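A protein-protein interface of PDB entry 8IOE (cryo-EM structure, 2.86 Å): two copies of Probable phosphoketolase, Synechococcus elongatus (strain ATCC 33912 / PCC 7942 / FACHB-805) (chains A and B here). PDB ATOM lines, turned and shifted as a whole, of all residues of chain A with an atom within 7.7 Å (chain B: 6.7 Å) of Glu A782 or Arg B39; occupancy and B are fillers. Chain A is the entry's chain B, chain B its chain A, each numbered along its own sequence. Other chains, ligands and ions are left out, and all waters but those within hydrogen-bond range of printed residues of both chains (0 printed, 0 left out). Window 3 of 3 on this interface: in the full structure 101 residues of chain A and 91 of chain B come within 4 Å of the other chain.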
ATOM      1  N   THR A 731      24.269  35.447  16.394  1.00  0.00           N
ATOM      2  CA  THR A 731      24.181  34.421  17.414  1.00  0.00           C
ATOM      3  C   THR A 731      24.911  34.889  18.670  1.00  0.00           C
ATOM      4  O   THR A 731      25.737  35.801  18.606  1.00  0.00           O
ATOM      5  CB  THR A 731      24.786  33.118  16.904  1.00  0.00           C
ATOM      6  OG1 THR A 731      26.213  33.200  16.969  1.00  0.00           O
ATOM      7  CG2 THR A 731      24.366  32.864  15.470  1.00  0.00           C
ATOM      8  N   ILE A 776      32.180  31.027  12.797  1.00  0.00           N
ATOM      9  CA  ILE A 776      31.429  32.008  12.022  1.00  0.00           C
ATOM     10  C   ILE A 776      30.847  31.367  10.769  1.00  0.00           C
ATOM     11  O   ILE A 776      29.690  31.615  10.410  1.00  0.00           O
ATOM     12  CB  ILE A 776      32.319  33.217  11.688  1.00  0.00           C
ATOM     13  CG1 ILE A 776      32.655  33.989  12.960  1.00  0.00           C
ATOM     14  CG2 ILE A 776      31.629  34.135  10.701  1.00  0.00           C
ATOM     15  CD1 ILE A 776      33.570  35.163  12.728  1.00  0.00           C
ATOM     16  N   GLN A 777      31.634  30.529  10.091  1.00  0.00           N
ATOM     17  CA  GLN A 777      31.136  29.849   8.900  1.00  0.00           C
ATOM     18  C   GLN A 777      29.989  28.909   9.237  1.00  0.00           C
ATOM     19  O   GLN A 777      29.005  28.828   8.493  1.00  0.00           O
ATOM     20  CB  GLN A 777      32.269  29.090   8.215  1.00  0.00           C
ATOM     21  CG  GLN A 777      33.276  29.989   7.534  1.00  0.00           C
ATOM     22  CD  GLN A 777      32.637  30.885   6.494  1.00  0.00           C
ATOM     23  OE1 GLN A 777      31.778  30.452   5.727  1.00  0.00           O
ATOM     24  NE2 GLN A 777      33.050  32.147   6.466  1.00  0.00           N
ATOM     25  N   TYR A 778      30.096  28.186  10.353  1.00  0.00           N
ATOM     26  CA  TYR A 778      28.996  27.331  10.781  1.00  0.00           C
ATOM     27  C   TYR A 778      27.773  28.159  11.149  1.00  0.00           C
ATOM     28  O   TYR A 778      26.634  27.730  10.931  1.00  0.00           O
ATOM     29  CB  TYR A 778      29.431  26.464  11.961  1.00  0.00           C
ATOM     30  CG  TYR A 778      28.391  25.458  12.397  1.00  0.00           C
ATOM     31  CD1 TYR A 778      28.319  24.208  11.804  1.00  0.00           C
ATOM     32  CD2 TYR A 778      27.484  25.758  13.404  1.00  0.00           C
ATOM     33  CE1 TYR A 778      27.374  23.287  12.199  1.00  0.00           C
ATOM     34  CE2 TYR A 778      26.536  24.844  13.804  1.00  0.00           C
ATOM     35  CZ  TYR A 778      26.486  23.610  13.199  1.00  0.00           C
ATOM     36  OH  TYR A 778      25.540  22.695  13.597  1.00  0.00           O
ATOM     37  N   ALA A 779      27.989  29.343  11.722  1.00  0.00           N
ATOM     38  CA  ALA A 779      26.874  30.206  12.089  1.00  0.00           C
ATOM     39  C   ALA A 779      26.117  30.691  10.860  1.00  0.00           C
ATOM     40  O   ALA A 779      24.888  30.796  10.885  1.00  0.00           O
ATOM     41  CB  ALA A 779      27.375  31.392  12.910  1.00  0.00           C
ATOM     42  N   TYR A 780      26.833  31.003   9.779  1.00  0.00           N
ATOM     43  CA  TYR A 780      26.162  31.485   8.576  1.00  0.00           C
ATOM     44  C   TYR A 780      25.355  30.382   7.906  1.00  0.00           C
ATOM     45  O   TYR A 780      24.269  30.638   7.375  1.00  0.00           O
ATOM     46  CB  TYR A 780      27.184  32.071   7.605  1.00  0.00           C
ATOM     47  CG  TYR A 780      27.688  33.433   8.010  1.00  0.00           C
ATOM     48  CD1 TYR A 780      26.982  34.210   8.918  1.00  0.00           C
ATOM     49  CD2 TYR A 780      28.864  33.945   7.486  1.00  0.00           C
ATOM     50  CE1 TYR A 780      27.435  35.456   9.294  1.00  0.00           C
ATOM     51  CE2 TYR A 780      29.325  35.191   7.856  1.00  0.00           C
ATOM     52  CZ  TYR A 780      28.605  35.943   8.760  1.00  0.00           C
ATOM     53  OH  TYR A 780      29.059  37.186   9.133  1.00  0.00           O
ATOM     54  N   GLN A 781      25.868  29.153   7.914  1.00  0.00           N
ATOM     55  CA  GLN A 781      25.168  28.060   7.248  1.00  0.00           C
ATOM     56  C   GLN A 781      23.959  27.595   8.048  1.00  0.00           C
ATOM     57  O   GLN A 781      22.902  27.309   7.474  1.00  0.00           O
ATOM     58  CB  GLN A 781      26.127  26.898   7.006  1.00  0.00           C
ATOM     59  CG  GLN A 781      27.316  27.254   6.140  1.00  0.00           C
ATOM     60  CD  GLN A 781      28.319  26.126   6.043  1.00  0.00           C
ATOM     61  OE1 GLN A 781      28.101  25.039   6.579  1.00  0.00           O
ATOM     62  NE2 GLN A 781      29.429  26.378   5.360  1.00  0.00           N
ATOM     63  N   GLU A 782      24.089  27.511   9.370  1.00  0.00           N
ATOM     64  CA  GLU A 782      23.053  26.917  10.203  1.00  0.00           C
ATOM     65  C   GLU A 782      22.209  27.935  10.952  1.00  0.00           C
ATOM     66  O   GLU A 782      21.038  27.663  11.228  1.00  0.00           O
ATOM     67  CB  GLU A 782      23.680  25.954  11.214  1.00  0.00           C
ATOM     68  CG  GLU A 782      24.531  24.866  10.584  1.00  0.00           C
ATOM     69  CD  GLU A 782      23.710  23.849   9.821  1.00  0.00           C
ATOM     70  OE1 GLU A 782      22.513  23.688  10.137  1.00  0.00           O
ATOM     71  OE2 GLU A 782      24.263  23.207   8.905  1.00  0.00           O
ATOM     72  N   GLY A 783      22.764  29.094  11.289  1.00  0.00           N
ATOM     73  CA  GLY A 783      22.040  30.072  12.071  1.00  0.00           C
ATOM     74  C   GLY A 783      22.077  29.849  13.564  1.00  0.00           C
ATOM     75  O   GLY A 783      21.494  30.649  14.305  1.00  0.00           O
ATOM     76  N   ILE A 784      22.738  28.789  14.029  1.00  0.00           N
ATOM     77  CA  ILE A 784      22.853  28.493  15.449  1.00  0.00           C
ATOM     78  C   ILE A 784      24.291  28.072  15.728  1.00  0.00           C
ATOM     79  O   ILE A 784      25.018  27.629  14.837  1.00  0.00           O
ATOM     80  CB  ILE A 784      21.850  27.397  15.890  1.00  0.00           C
ATOM     81  CG1 ILE A 784      21.656  27.401  17.408  1.00  0.00           C
ATOM     82  CG2 ILE A 784      22.294  26.026  15.405  1.00  0.00           C
ATOM     83  CD1 ILE A 784      21.260  28.746  17.967  1.00  0.00           C
ATOM     84  N   ASP A 785      24.705  28.240  16.979  1.00  0.00           N
ATOM     85  CA  ASP A 785      26.043  27.843  17.381  1.00  0.00           C
ATOM     86  C   ASP A 785      26.168  26.324  17.408  1.00  0.00           C
ATOM     87  O   ASP A 785      25.177  25.590  17.408  1.00  0.00           O
ATOM     88  CB  ASP A 785      26.379  28.417  18.754  1.00  0.00           C
ATOM     89  CG  ASP A 785      26.269  29.924  18.795  1.00  0.00           C
ATOM     90  OD1 ASP A 785      26.624  30.569  17.787  1.00  0.00           O
ATOM     91  OD2 ASP A 785      25.828  30.465  19.831  1.00  0.00           O
ATOM     92  N   ARG A 786      27.412  25.857  17.423  1.00  0.00           N
ATOM     93  CA  ARG A 786      27.670  24.432  17.523  1.00  0.00           C
ATOM     94  C   ARG A 786      27.190  23.907  18.875  1.00  0.00           C
ATOM     95  O   ARG A 786      27.177  24.643  19.864  1.00  0.00           O
ATOM     96  CB  ARG A 786      29.157  24.145  17.344  1.00  0.00           C
ATOM     97  CG  ARG A 786      29.682  24.466  15.959  1.00  0.00           C
ATOM     98  CD  ARG A 786      31.139  24.066  15.817  1.00  0.00           C
ATOM     99  NE  ARG A 786      31.644  24.312  14.473  1.00  0.00           N
ATOM    100  CZ  ARG A 786      31.570  23.442  13.476  1.00  0.00           C
ATOM    101  NH1 ARG A 786      31.013  22.253  13.635  1.00  0.00           N
ATOM    102  NH2 ARG A 786      32.067  23.773  12.288  1.00  0.00           N
ATOM    103  N   GLY B  34       6.457  32.043   6.491  1.00  0.00           N
ATOM    104  CA  GLY B  34       7.519  31.365   5.769  1.00  0.00           C
ATOM    105  C   GLY B  34       8.895  31.833   6.196  1.00  0.00           C
ATOM    106  O   GLY B  34       9.793  31.027   6.444  1.00  0.00           O
ATOM    107  N   GLN B  35       9.077  33.149   6.298  1.00  0.00           N
ATOM    108  CA  GLN B  35      10.369  33.675   6.718  1.00  0.00           C
ATOM    109  C   GLN B  35      10.593  33.516   8.214  1.00  0.00           C
ATOM    110  O   GLN B  35      11.743  33.454   8.658  1.00  0.00           O
ATOM    111  CB  GLN B  35      10.496  35.141   6.308  1.00  0.00           C
ATOM    112  CG  GLN B  35       9.303  35.993   6.665  1.00  0.00           C
ATOM    113  CD  GLN B  35       9.313  37.317   5.938  1.00  0.00           C
ATOM    114  OE1 GLN B  35      10.347  37.759   5.441  1.00  0.00           O
ATOM    115  NE2 GLN B  35       8.157  37.964   5.876  1.00  0.00           N
ATOM    116  N   TYR B  37       9.626  30.808   9.933  1.00  0.00           N
ATOM    117  CA  TYR B  37       9.889  29.399  10.189  1.00  0.00           C
ATOM    118  C   TYR B  37      10.736  28.743   9.107  1.00  0.00           C
ATOM    119  O   TYR B  37      11.794  28.184   9.405  1.00  0.00           O
ATOM    120  CB  TYR B  37       8.564  28.645  10.334  1.00  0.00           C
ATOM    121  CG  TYR B  37       7.802  28.980  11.585  1.00  0.00           C
ATOM    122  CD1 TYR B  37       8.178  28.446  12.806  1.00  0.00           C
ATOM    123  CD2 TYR B  37       6.702  29.821  11.547  1.00  0.00           C
ATOM    124  CE1 TYR B  37       7.484  28.742  13.952  1.00  0.00           C
ATOM    125  CE2 TYR B  37       6.000  30.122  12.691  1.00  0.00           C
ATOM    126  CZ  TYR B  37       6.398  29.579  13.890  1.00  0.00           C
ATOM    127  OH  TYR B  37       5.709  29.870  15.038  1.00  0.00           O
ATOM    128  N   LEU B  38      10.294  28.789   7.855  1.00  0.00           N
ATOM    129  CA  LEU B  38      10.896  27.955   6.824  1.00  0.00           C
ATOM    130  C   LEU B  38      12.273  28.470   6.432  1.00  0.00           C
ATOM    131  O   LEU B  38      12.465  29.669   6.213  1.00  0.00           O
ATOM    132  CB  LEU B  38       9.992  27.893   5.596  1.00  0.00           C
ATOM    133  CG  LEU B  38       8.565  27.407   5.838  1.00  0.00           C
ATOM    134  CD1 LEU B  38       7.839  27.227   4.519  1.00  0.00           C
ATOM    135  CD2 LEU B  38       8.571  26.115   6.629  1.00  0.00           C
ATOM    136  N   ARG B  39      13.232  27.554   6.354  1.00  0.00           N
ATOM    137  CA  ARG B  39      14.552  27.829   5.806  1.00  0.00           C
ATOM    138  C   ARG B  39      14.710  27.302   4.390  1.00  0.00           C
ATOM    139  O   ARG B  39      15.403  27.923   3.578  1.00  0.00           O
ATOM    140  CB  ARG B  39      15.627  27.214   6.709  1.00  0.00           C
ATOM    141  CG  ARG B  39      17.051  27.425   6.239  1.00  0.00           C
ATOM    142  CD  ARG B  39      18.040  26.908   7.263  1.00  0.00           C
ATOM    143  NE  ARG B  39      17.799  25.509   7.591  1.00  0.00           N
ATOM    144  CZ  ARG B  39      18.512  24.812   8.465  1.00  0.00           C
ATOM    145  NH1 ARG B  39      19.524  25.354   9.119  1.00  0.00           N
ATOM    146  NH2 ARG B  39      18.201  23.538   8.686  1.00  0.00           N
ATOM    147  N   ASP B  40      14.062  26.184   4.074  1.00  0.00           N
ATOM    148  CA  ASP B  40      14.060  25.614   2.738  1.00  0.00           C
ATOM    149  C   ASP B  40      12.643  25.151   2.428  1.00  0.00           C
ATOM    150  O   ASP B  40      11.757  25.195   3.287  1.00  0.00           O
ATOM    151  CB  ASP B  40      15.062  24.457   2.624  1.00  0.00           C
ATOM    152  CG  ASP B  40      15.448  24.155   1.191  1.00  0.00           C
ATOM    153  OD1 ASP B  40      14.903  24.812   0.280  1.00  0.00           O
ATOM    154  OD2 ASP B  40      16.291  23.260   0.978  1.00  0.00           O
ATOM    155  N   ASN B  41      12.436  24.705   1.183  1.00  0.00           N
ATOM    156  CA  ASN B  41      11.148  24.242   0.676  1.00  0.00           C
ATOM    157  C   ASN B  41      10.095  25.331   0.853  1.00  0.00           C
ATOM    158  O   ASN B  41       9.201  25.202   1.700  1.00  0.00           O
ATOM    159  CB  ASN B  41      10.721  22.949   1.377  1.00  0.00           C
ATOM    160  CG  ASN B  41       9.497  22.320   0.746  1.00  0.00           C
ATOM    161  OD1 ASN B  41       9.232  22.502  -0.441  1.00  0.00           O
ATOM    162  ND2 ASN B  41       8.739  21.577   1.542  1.00  0.00           N
ATOM    163  N   PRO B  42      10.177  26.423   0.089  1.00  0.00           N
ATOM    164  CA  PRO B  42       9.264  27.549   0.344  1.00  0.00           C
ATOM    165  C   PRO B  42       7.826  27.267  -0.050  1.00  0.00           C
ATOM    166  O   PRO B  42       6.905  27.718   0.642  1.00  0.00           O
ATOM    167  CB  PRO B  42       9.875  28.678  -0.494  1.00  0.00           C
ATOM    168  CG  PRO B  42      10.552  27.971  -1.619  1.00  0.00           C
ATOM    169  CD  PRO B  42      11.074  26.681  -1.050  1.00  0.00           C
ATOM    170  N   PRO B  50      12.038  18.610   9.486  1.00  0.00           N
ATOM    171  CA  PRO B  50      12.685  19.532  10.437  1.00  0.00           C
ATOM    172  C   PRO B  50      13.868  20.299   9.870  1.00  0.00           C
ATOM    173  O   PRO B  50      14.153  21.404  10.348  1.00  0.00           O
ATOM    174  CB  PRO B  50      13.116  18.603  11.578  1.00  0.00           C
ATOM    175  CG  PRO B  50      12.146  17.485  11.523  1.00  0.00           C
ATOM    176  CD  PRO B  50      11.868  17.265  10.066  1.00  0.00           C
ATOM    177  N   GLU B  51      14.569  19.759   8.871  1.00  0.00           N
ATOM    178  CA  GLU B  51      15.699  20.488   8.304  1.00  0.00           C
ATOM    179  C   GLU B  51      15.265  21.719   7.519  1.00  0.00           C
ATOM    180  O   GLU B  51      16.110  22.564   7.204  1.00  0.00           O
ATOM    181  CB  GLU B  51      16.536  19.573   7.410  1.00  0.00           C
ATOM    182  CG  GLU B  51      15.792  18.987   6.226  1.00  0.00           C
ATOM    183  CD  GLU B  51      15.168  17.644   6.540  1.00  0.00           C
ATOM    184  OE1 GLU B  51      14.898  17.371   7.729  1.00  0.00           O
ATOM    185  OE2 GLU B  51      14.951  16.857   5.596  1.00  0.00           O
ATOM    186  N   HIS B  52      13.979  21.841   7.192  1.00  0.00           N
ATOM    187  CA  HIS B  52      13.471  23.042   6.546  1.00  0.00           C
ATOM    188  C   HIS B  52      13.156  24.158   7.533  1.00  0.00           C
ATOM    189  O   HIS B  52      12.901  25.287   7.103  1.00  0.00           O
ATOM    190  CB  HIS B  52      12.211  22.721   5.742  1.00  0.00           C
ATOM    191  CG  HIS B  52      12.393  21.622   4.743  1.00  0.00           C
ATOM    192  ND1 HIS B  52      13.174  21.761   3.617  1.00  0.00           N
ATOM    193  CD2 HIS B  52      11.885  20.368   4.697  1.00  0.00           C
ATOM    194  CE1 HIS B  52      13.144  20.639   2.923  1.00  0.00           C
ATOM    195  NE2 HIS B  52      12.369  19.777   3.556  1.00  0.00           N
ATOM    196  N   ILE B  53      13.164  23.876   8.830  1.00  0.00           N
ATOM    197  CA  ILE B  53      12.772  24.838   9.853  1.00  0.00           C
ATOM    198  C   ILE B  53      14.023  25.478  10.436  1.00  0.00           C
ATOM    199  O   ILE B  53      15.045  24.808  10.628  1.00  0.00           O
ATOM    200  CB  ILE B  53      11.930  24.161  10.950  1.00  0.00           C
ATOM    201  CG1 ILE B  53      10.830  23.308  10.322  1.00  0.00           C
ATOM    202  CG2 ILE B  53      11.314  25.194  11.873  1.00  0.00           C
ATOM    203  CD1 ILE B  53       9.865  24.095   9.475  1.00  0.00           C
ATOM    204  N   LYS B  54      13.947  26.778  10.708  1.00  0.00           N
ATOM    205  CA  LYS B  54      15.057  27.481  11.335  1.00  0.00           C
ATOM    206  C   LYS B  54      15.271  26.982  12.757  1.00  0.00           C
ATOM    207  O   LYS B  54      14.315  26.726  13.493  1.00  0.00           O
ATOM    208  CB  LYS B  54      14.797  28.984  11.344  1.00  0.00           C
ATOM    209  CG  LYS B  54      14.749  29.612   9.966  1.00  0.00           C
ATOM    210  CD  LYS B  54      14.482  31.102  10.053  1.00  0.00           C
ATOM    211  CE  LYS B  54      14.601  31.758   8.692  1.00  0.00           C
ATOM    212  NZ  LYS B  54      13.670  31.159   7.701  1.00  0.00           N
ATOM    213  N   GLN B  55      16.542  26.840  13.139  1.00  0.00           N
ATOM    214  CA  GLN B  55      16.866  26.322  14.464  1.00  0.00           C
ATOM    215  C   GLN B  55      16.451  27.299  15.558  1.00  0.00           C
ATOM    216  O   GLN B  55      15.862  26.900  16.569  1.00  0.00           O
ATOM    217  CB  GLN B  55      18.361  26.013  14.556  1.00  0.00           C
ATOM    218  CG  GLN B  55      18.788  24.727  13.858  1.00  0.00           C
ATOM    219  CD  GLN B  55      18.793  24.842  12.344  1.00  0.00           C
ATOM    220  OE1 GLN B  55      18.672  25.934  11.790  1.00  0.00           O
ATOM    221  NE2 GLN B  55      18.934  23.709  11.668  1.00  0.00           N
ATOM    222  N   ARG B  56      16.745  28.581  15.373  1.00  0.00           N
ATOM    223  CA  ARG B  56      16.405  29.614  16.339  1.00  0.00           C
ATOM    224  C   ARG B  56      15.323  30.508  15.753  1.00  0.00           C
ATOM    225  O   ARG B  56      15.479  31.031  14.646  1.00  0.00           O
ATOM    226  CB  ARG B  56      17.637  30.441  16.713  1.00  0.00           C
ATOM    227  CG  ARG B  56      17.389  31.451  17.818  1.00  0.00           C
ATOM    228  CD  ARG B  56      18.649  32.230  18.147  1.00  0.00           C
ATOM    229  NE  ARG B  56      19.169  32.936  16.983  1.00  0.00           N
ATOM    230  CZ  ARG B  56      20.186  33.786  17.014  1.00  0.00           C
ATOM    231  NH1 ARG B  56      20.816  34.067  18.141  1.00  0.00           N
ATOM    232  NH2 ARG B  56      20.577  34.371  15.886  1.00  0.00           N
ATOM    233  N   LEU B 122      12.258  32.747  -3.507  1.00  0.00           N
ATOM    234  CA  LEU B 122      11.458  32.520  -2.309  1.00  0.00           C
ATOM    235  C   LEU B 122      12.253  31.771  -1.251  1.00  0.00           C
ATOM    236  O   LEU B 122      12.121  32.047  -0.053  1.00  0.00           O
ATOM    237  CB  LEU B 122      10.187  31.753  -2.662  1.00  0.00           C
ATOM    238  CG  LEU B 122       8.990  32.621  -3.032  1.00  0.00           C
ATOM    239  CD1 LEU B 122       7.810  31.756  -3.430  1.00  0.00           C
ATOM    240  CD2 LEU B 122       8.634  33.515  -1.861  1.00  0.00           C
ATOM    241  N   GLN B 123      13.070  30.805  -1.675  1.00  0.00           N
ATOM    242  CA  GLN B 123      13.941  30.112  -0.735  1.00  0.00           C
ATOM    243  C   GLN B 123      14.947  31.073  -0.119  1.00  0.00           C
ATOM    244  O   GLN B 123      15.224  31.006   1.084  1.00  0.00           O
ATOM    245  CB  GLN B 123      14.652  28.955  -1.439  1.00  0.00           C
ATOM    246  CG  GLN B 123      15.381  27.999  -0.509  1.00  0.00           C
ATOM    247  CD  GLN B 123      16.804  28.431  -0.218  1.00  0.00           C
ATOM    248  OE1 GLN B 123      17.358  29.285  -0.909  1.00  0.00           O
ATOM    249  NE2 GLN B 123      17.402  27.844   0.810  1.00  0.00           N
ATOM    250  N   GLN B 124      15.502  31.976  -0.927  1.00  0.00           N
ATOM    251  CA  GLN B 124      16.436  32.966  -0.403  1.00  0.00           C
ATOM    252  C   GLN B 124      15.724  33.993   0.468  1.00  0.00           C
ATOM    253  O   GLN B 124      16.282  34.462   1.467  1.00  0.00           O
ATOM    254  CB  GLN B 124      17.169  33.651  -1.554  1.00  0.00           C
ATOM    255  CG  GLN B 124      18.253  34.614  -1.111  1.00  0.00           C
ATOM    256  CD  GLN B 124      19.371  33.923  -0.357  1.00  0.00           C
ATOM    257  OE1 GLN B 124      19.708  32.774  -0.641  1.00  0.00           O
ATOM    258  NE2 GLN B 124      19.949  34.620   0.612  1.00  0.00           N
ATOM    259  N   PHE B 126      13.042  33.596   2.406  1.00  0.00           N
ATOM    260  CA  PHE B 126      12.789  33.038   3.729  1.00  0.00           C
ATOM    261  C   PHE B 126      14.085  32.840   4.503  1.00  0.00           C
ATOM    262  O   PHE B 126      14.125  33.037   5.723  1.00  0.00           O
ATOM    263  CB  PHE B 126      12.038  31.714   3.607  1.00  0.00           C
ATOM    264  CG  PHE B 126      10.637  31.854   3.097  1.00  0.00           C
ATOM    265  CD1 PHE B 126       9.965  33.056   3.196  1.00  0.00           C
ATOM    266  CD2 PHE B 126       9.990  30.777   2.521  1.00  0.00           C
ATOM    267  CE1 PHE B 126       8.673  33.182   2.731  1.00  0.00           C
ATOM    268  CE2 PHE B 126       8.700  30.898   2.053  1.00  0.00           C
ATOM    269  CZ  PHE B 126       8.042  32.100   2.157  1.00  0.00           C
ATOM    270  N   LYS B 127      15.151  32.442   3.807  1.00  0.00           N
ATOM    271  CA  LYS B 127      16.409  32.114   4.468  1.00  0.00           C
ATOM    272  C   LYS B 127      17.036  33.336   5.127  1.00  0.00           C
ATOM    273  O   LYS B 127      17.576  33.239   6.235  1.00  0.00           O
ATOM    274  CB  LYS B 127      17.371  31.496   3.454  1.00  0.00           C
ATOM    275  CG  LYS B 127      18.805  31.353   3.923  1.00  0.00           C
ATOM    276  CD  LYS B 127      18.932  30.346   5.044  1.00  0.00           C
ATOM    277  CE  LYS B 127      20.365  29.861   5.172  1.00  0.00           C
ATOM    278  NZ  LYS B 127      21.325  30.996   5.223  1.00  0.00           N
ATOM    279  N   PHE B 131      18.347  35.747  10.362  1.00  0.00           N
ATOM    280  CA  PHE B 131      19.497  34.885  10.163  1.00  0.00           C
ATOM    281  C   PHE B 131      20.774  35.705  10.225  1.00  0.00           C
ATOM    282  O   PHE B 131      20.765  36.897   9.901  1.00  0.00           O
ATOM    283  CB  PHE B 131      19.413  34.170   8.808  1.00  0.00           C
ATOM    284  CG  PHE B 131      19.758  32.716   8.869  1.00  0.00           C
ATOM    285  CD1 PHE B 131      18.850  31.800   9.366  1.00  0.00           C
ATOM    286  CD2 PHE B 131      20.984  32.262   8.422  1.00  0.00           C
ATOM    287  CE1 PHE B 131      19.161  30.458   9.423  1.00  0.00           C
ATOM    288  CE2 PHE B 131      21.302  30.922   8.478  1.00  0.00           C
ATOM    289  CZ  PHE B 131      20.388  30.019   8.975  1.00  0.00           C
ATOM    290  N   PRO B 132      21.877  35.103  10.668  1.00  0.00           N
ATOM    291  CA  PRO B 132      23.175  35.775  10.551  1.00  0.00           C
ATOM    292  C   PRO B 132      23.482  36.103   9.099  1.00  0.00           C
ATOM    293  O   PRO B 132      23.268  35.289   8.199  1.00  0.00           O
ATOM    294  CB  PRO B 132      24.156  34.746  11.119  1.00  0.00           C
ATOM    295  CG  PRO B 132      23.337  33.932  12.050  1.00  0.00           C
ATOM    296  CD  PRO B 132      21.970  33.853  11.438  1.00  0.00           C
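The side-chain amide oxygen (OE1) of Gln B55 sits close to the backbone carbonyl oxygen (O) of Glu A782 (3.0 Å). The guanidinium group of Arg B39 lies within salt-bridge range of the side-chain carboxylate of Glu A782 (3.6 Å).
OE1 of Gln B55 sits at hydrogen-bond distance from NH1 of Arg B39 (2.9 Å). The backbone carbonyl oxygen (O) of Glu B51 lies within hydrogen-bond range of the guanidinium group (NH2) of Arg B39, at 2.7 Å. The side-chain hydroxyl of Thr A731 is in hydrogen-bond range of the side-chain carboxylate of Asp A785, 2.8 Å away. The backbone NH (N) of Arg B39 is in hydrogen-bond range of the backbone carbonyl oxygen (O) of His B52 (2.4 Å). The backbone carbonyl oxygen of Arg B39 lies within hydrogen-bond range of the side-chain amide nitrogen of Gln B123 (3.4 Å).
Among the printed residues, pairs that only touch across the chains: Tyr A780 with Phe B131, Glu A782 with Phe B131, Gly A783 with Phe B131, Thr A731 with Arg B56, Tyr A780 with Pro B132, Tyr A780 with Lys B127, Ala A779 with Pro B132, Thr A731 with Pro B132, Gly A783 with Pro B132, Ile A784 with Gln B55 and Gln A781 with Phe B131.
Gln A777 touches none of the printed residues of chain B. Of the printed residues of chain B, Ala A779 touches Pro B132. Printed residues of chain B within 4 Å of Tyr A780: Lys B127 (3.7 Å), Phe B131 (3.2 Å) and Pro B132 (3.6 Å). Of chain B, only Arg B39, Gln B55 and Phe B131 come within 4 Å of Glu A782. Gln B35 touches none of the printed residues of chain A. Arg B39 touches just one residue of chain A: Glu A782 (3.5 Å). The nearest residue of chain B that does not touch Glu A782 is Pro B132 (5.9 Å). The nearest printed residue of chain A that does not touch Lys B127 is Gln A781 (4.3 Å).
Of the 22 printed residues of chain B, 6 touch a printed residue of chain A. Printed residues of chain B that touch a printed residue of chain A: Arg B39, Gln B55, Arg B56, Lys B127, Phe B131 and Pro B132. Among the printed residues, Asp or Glu carboxylates within 4 Å of a Lys or Arg side-chain nitrogen of the other chain: Glu A782 with Arg B39 (3.6 Å).
No position is printed for both chains. Of the 13 pairs that touch across the chains among the printed residues, none has its exchanged pair printed and touching as well.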
